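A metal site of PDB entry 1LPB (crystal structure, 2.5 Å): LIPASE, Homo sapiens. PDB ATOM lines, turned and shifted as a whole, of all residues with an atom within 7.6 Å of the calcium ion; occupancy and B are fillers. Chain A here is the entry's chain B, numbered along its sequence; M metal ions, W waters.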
ATOM      1  N   HIS A 157       5.142 -22.507   0.556  1.00  0.00           N
ATOM      2  CA  HIS A 157       6.334 -23.057   1.188  1.00  0.00           C
ATOM      3  C   HIS A 157       7.447 -23.326   0.179  1.00  0.00           C
ATOM      4  O   HIS A 157       8.628 -23.301   0.545  1.00  0.00           O
ATOM      5  CB  HIS A 157       5.970 -24.300   1.985  1.00  0.00           C
ATOM      6  CG  HIS A 157       4.969 -24.039   3.071  1.00  0.00           C
ATOM      7  ND1 HIS A 157       5.183 -23.138   4.083  1.00  0.00           N
ATOM      8  CD2 HIS A 157       3.725 -24.541   3.281  1.00  0.00           C
ATOM      9  CE1 HIS A 157       4.127 -23.089   4.870  1.00  0.00           C
ATOM     10  NE2 HIS A 157       3.232 -23.936   4.405  1.00  0.00           N
ATOM     11  N   ALA A 159       7.921 -21.366  -2.263  1.00  0.00           N
ATOM     12  CA  ALA A 159       8.407 -19.977  -2.375  1.00  0.00           C
ATOM     13  C   ALA A 159       9.353 -19.662  -1.193  1.00  0.00           C
ATOM     14  O   ALA A 159      10.334 -18.934  -1.357  1.00  0.00           O
ATOM     15  CB  ALA A 159       7.237 -19.000  -2.389  1.00  0.00           C
ATOM     16  N   GLY A 160       9.053 -20.225  -0.024  1.00  0.00           N
ATOM     17  CA  GLY A 160       9.889 -20.033   1.132  1.00  0.00           C
ATOM     18  C   GLY A 160      11.170 -20.852   1.036  1.00  0.00           C
ATOM     19  O   GLY A 160      12.176 -20.540   1.689  1.00  0.00           O
ATOM     20  N   GLU A 161      11.116 -21.956   0.305  1.00  0.00           N
ATOM     21  CA  GLU A 161      12.289 -22.807   0.126  1.00  0.00           C
ATOM     22  C   GLU A 161      13.238 -22.109  -0.865  1.00  0.00           C
ATOM     23  O   GLU A 161      14.461 -22.090  -0.665  1.00  0.00           O
ATOM     24  CB  GLU A 161      11.868 -24.199  -0.383  1.00  0.00           C
ATOM     25  CG  GLU A 161      13.020 -25.076  -0.908  1.00  0.00           C
ATOM     26  CD  GLU A 161      14.105 -25.406   0.113  1.00  0.00           C
ATOM     27  OE1 GLU A 161      13.857 -25.257   1.322  1.00  0.00           O
ATOM     28  OE2 GLU A 161      15.208 -25.815  -0.299  1.00  0.00           O
ATOM     29  N   GLY A 163      13.457 -18.977  -1.171  1.00  0.00           N
ATOM     30  CA  GLY A 163      14.021 -17.795  -0.507  1.00  0.00           C
ATOM     31  C   GLY A 163      15.135 -18.171   0.456  1.00  0.00           C
ATOM     32  O   GLY A 163      16.072 -17.407   0.692  1.00  0.00           O
ATOM     33  N   ARG A 164      15.024 -19.359   1.035  1.00  0.00           N
ATOM     34  CA  ARG A 164      16.031 -19.847   1.950  1.00  0.00           C
ATOM     35  C   ARG A 164      17.337 -19.914   1.165  1.00  0.00           C
ATOM     36  O   ARG A 164      18.352 -19.309   1.524  1.00  0.00           O
ATOM     37  CB  ARG A 164      15.648 -21.254   2.402  1.00  0.00           C
ATOM     38  CG  ARG A 164      16.330 -21.734   3.681  1.00  0.00           C
ATOM     39  CD  ARG A 164      16.306 -23.247   3.753  1.00  0.00           C
ATOM     40  NE  ARG A 164      17.479 -23.795   3.089  1.00  0.00           N
ATOM     41  CZ  ARG A 164      17.510 -24.897   2.359  1.00  0.00           C
ATOM     42  NH1 ARG A 164      16.422 -25.635   2.191  1.00  0.00           N
ATOM     43  NH2 ARG A 164      18.644 -25.278   1.817  1.00  0.00           N
ATOM     44  N   PRO A 187       9.936 -26.072  12.242  1.00  0.00           N
ATOM     45  CA  PRO A 187      10.951 -25.008  12.172  1.00  0.00           C
ATOM     46  C   PRO A 187      10.953 -24.210  10.860  1.00  0.00           C
ATOM     47  O   PRO A 187      10.569 -24.698   9.808  1.00  0.00           O
ATOM     48  CB  PRO A 187      12.274 -25.785  12.364  1.00  0.00           C
ATOM     49  CG  PRO A 187      11.840 -26.976  13.222  1.00  0.00           C
ATOM     50  CD  PRO A 187      10.537 -27.375  12.571  1.00  0.00           C
ATOM     51  N   GLU A 188      11.466 -22.993  10.896  1.00  0.00           N
ATOM     52  CA  GLU A 188      11.492 -22.129   9.710  1.00  0.00           C
ATOM     53  C   GLU A 188      12.210 -22.696   8.491  1.00  0.00           C
ATOM     54  O   GLU A 188      11.985 -22.229   7.341  1.00  0.00           O
ATOM     55  CB  GLU A 188      12.117 -20.792  10.077  1.00  0.00           C
ATOM     56  CG  GLU A 188      11.373 -20.036  11.161  1.00  0.00           C
ATOM     57  CD  GLU A 188      12.128 -20.006  12.445  1.00  0.00           C
ATOM     58  OE1 GLU A 188      12.961 -19.094  12.595  1.00  0.00           O
ATOM     59  OE2 GLU A 188      11.873 -20.883  13.308  1.00  0.00           O
ATOM     60  N   LEU A 189      13.122 -23.635   8.730  1.00  0.00           N
ATOM     61  CA  LEU A 189      13.902 -24.269   7.663  1.00  0.00           C
ATOM     62  C   LEU A 189      12.980 -24.935   6.674  1.00  0.00           C
ATOM     63  O   LEU A 189      13.122 -24.819   5.478  1.00  0.00           O
ATOM     64  CB  LEU A 189      14.829 -25.327   8.249  1.00  0.00           C
ATOM     65  CG  LEU A 189      15.672 -26.155   7.271  1.00  0.00           C
ATOM     66  CD1 LEU A 189      16.913 -25.356   6.810  1.00  0.00           C
ATOM     67  CD2 LEU A 189      16.105 -27.465   7.917  1.00  0.00           C
ATOM     68  N   VAL A 190      11.966 -25.556   7.244  1.00  0.00           N
ATOM     69  CA  VAL A 190      10.967 -26.337   6.566  1.00  0.00           C
ATOM     70  C   VAL A 190       9.706 -25.614   6.023  1.00  0.00           C
ATOM     71  O   VAL A 190       8.948 -26.177   5.226  1.00  0.00           O
ATOM     72  CB  VAL A 190      10.623 -27.451   7.545  1.00  0.00           C
ATOM     73  CG1 VAL A 190       9.378 -28.222   7.133  1.00  0.00           C
ATOM     74  CG2 VAL A 190      11.868 -28.361   7.708  1.00  0.00           C
ATOM     75  N   ARG A 191       9.542 -24.327   6.350  1.00  0.00           N
ATOM     76  CA  ARG A 191       8.362 -23.550   5.927  1.00  0.00           C
ATOM     77  C   ARG A 191       8.674 -22.073   5.700  1.00  0.00           C
ATOM     78  O   ARG A 191       9.787 -21.576   5.974  1.00  0.00           O
ATOM     79  CB  ARG A 191       7.326 -23.607   7.054  1.00  0.00           C
ATOM     80  CG  ARG A 191       7.982 -23.504   8.423  1.00  0.00           C
ATOM     81  CD  ARG A 191       7.048 -23.144   9.546  1.00  0.00           C
ATOM     82  NE  ARG A 191       6.924 -21.702   9.606  1.00  0.00           N
ATOM     83  CZ  ARG A 191       7.294 -20.943  10.643  1.00  0.00           C
ATOM     84  NH1 ARG A 191       7.768 -21.498  11.754  1.00  0.00           N
ATOM     85  NH2 ARG A 191       7.145 -19.618  10.564  1.00  0.00           N
ATOM     86  N   LEU A 192       7.652 -21.362   5.231  1.00  0.00           N
ATOM     87  CA  LEU A 192       7.722 -19.931   4.986  1.00  0.00           C
ATOM     88  C   LEU A 192       7.832 -19.289   6.355  1.00  0.00           C
ATOM     89  O   LEU A 192       7.325 -19.846   7.320  1.00  0.00           O
ATOM     90  CB  LEU A 192       6.423 -19.452   4.384  1.00  0.00           C
ATOM     91  CG  LEU A 192       6.320 -17.966   4.024  1.00  0.00           C
ATOM     92  CD1 LEU A 192       7.340 -17.625   2.967  1.00  0.00           C
ATOM     93  CD2 LEU A 192       4.934 -17.679   3.515  1.00  0.00           C
ATOM     94  N   ASP A 193       8.589 -18.194   6.445  1.00  0.00           N
ATOM     95  CA  ASP A 193       8.775 -17.402   7.666  1.00  0.00           C
ATOM     96  C   ASP A 193       9.342 -16.119   7.130  1.00  0.00           C
ATOM     97  O   ASP A 193       9.913 -16.116   6.045  1.00  0.00           O
ATOM     98  CB  ASP A 193       9.726 -18.058   8.671  1.00  0.00           C
ATOM     99  CG  ASP A 193      11.119 -18.180   8.150  1.00  0.00           C
ATOM    100  OD1 ASP A 193      11.450 -19.189   7.511  1.00  0.00           O
ATOM    101  OD2 ASP A 193      11.884 -17.251   8.376  1.00  0.00           O
ATOM    102  N   PRO A 194       9.265 -15.035   7.892  1.00  0.00           N
ATOM    103  CA  PRO A 194       9.761 -13.712   7.468  1.00  0.00           C
ATOM    104  C   PRO A 194      11.183 -13.643   6.894  1.00  0.00           C
ATOM    105  O   PRO A 194      11.463 -12.801   6.029  1.00  0.00           O
ATOM    106  CB  PRO A 194       9.648 -12.897   8.739  1.00  0.00           C
ATOM    107  CG  PRO A 194       8.525 -13.554   9.487  1.00  0.00           C
ATOM    108  CD  PRO A 194       8.816 -14.999   9.294  1.00  0.00           C
ATOM    109  N   SER A 195      12.074 -14.529   7.367  1.00  0.00           N
ATOM    110  CA  SER A 195      13.474 -14.518   6.922  1.00  0.00           C
ATOM    111  C   SER A 195      13.785 -14.978   5.485  1.00  0.00           C
ATOM    112  O   SER A 195      14.925 -14.769   5.016  1.00  0.00           O
ATOM    113  CB  SER A 195      14.335 -15.326   7.894  1.00  0.00           C
ATOM    114  OG  SER A 195      14.155 -16.711   7.664  1.00  0.00           O
ATOM    115  N   ASP A 196      12.833 -15.619   4.803  1.00  0.00           N
ATOM    116  CA  ASP A 196      13.055 -16.104   3.436  1.00  0.00           C
ATOM    117  C   ASP A 196      13.111 -15.014   2.373  1.00  0.00           C
ATOM    118  O   ASP A 196      13.632 -15.248   1.287  1.00  0.00           O
ATOM    119  CB  ASP A 196      11.955 -17.121   3.045  1.00  0.00           C
ATOM    120  CG  ASP A 196      11.937 -18.368   3.922  1.00  0.00           C
ATOM    121  OD1 ASP A 196      12.970 -18.819   4.423  1.00  0.00           O
ATOM    122  OD2 ASP A 196      10.869 -18.948   4.063  1.00  0.00           O
ATOM    123  N   ALA A 197      12.586 -13.832   2.657  1.00  0.00           N
ATOM    124  CA  ALA A 197      12.566 -12.766   1.657  1.00  0.00           C
ATOM    125  C   ALA A 197      12.802 -11.439   2.358  1.00  0.00           C
ATOM    126  O   ALA A 197      12.637 -11.336   3.575  1.00  0.00           O
ATOM    127  CB  ALA A 197      11.228 -12.750   0.962  1.00  0.00           C
HETATM  128 CA    CA M   1      11.813 -20.581   5.766  1.00  0.00          CA
HETATM  129  O   HOH W   1      12.189 -22.040   4.190  1.00  0.00           O
HETATM  130  O   HOH W   2      13.941 -20.819   6.361  1.00  0.00           O
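OD2 of Asp 193 sits at hydrogen-bond distance from OG of Ser 195.
Of the 17 residues printed, 4 come within 4 Å of the calcium ion.
The calcium ion is bound by water W1 (2.2 Å), water W2 (2.2 Å), the side-chain carboxylate (OD1) of Asp 193 (2.3 Å), the backbone carbonyl oxygen (O) of Arg 191 (2.3 Å), the backbone carbonyl oxygen (O) of Glu 188 (2.3 Å), the side-chain carboxylate (OD1) of Asp 196 (2.5 Å) and the side-chain carboxylate (OD2) of Asp 196 (2.5 Å).
Water W1 lies within hydrogen-bond range of O of Gly 160 (2.9 Å) and O of Leu 189 (3.2 Å).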
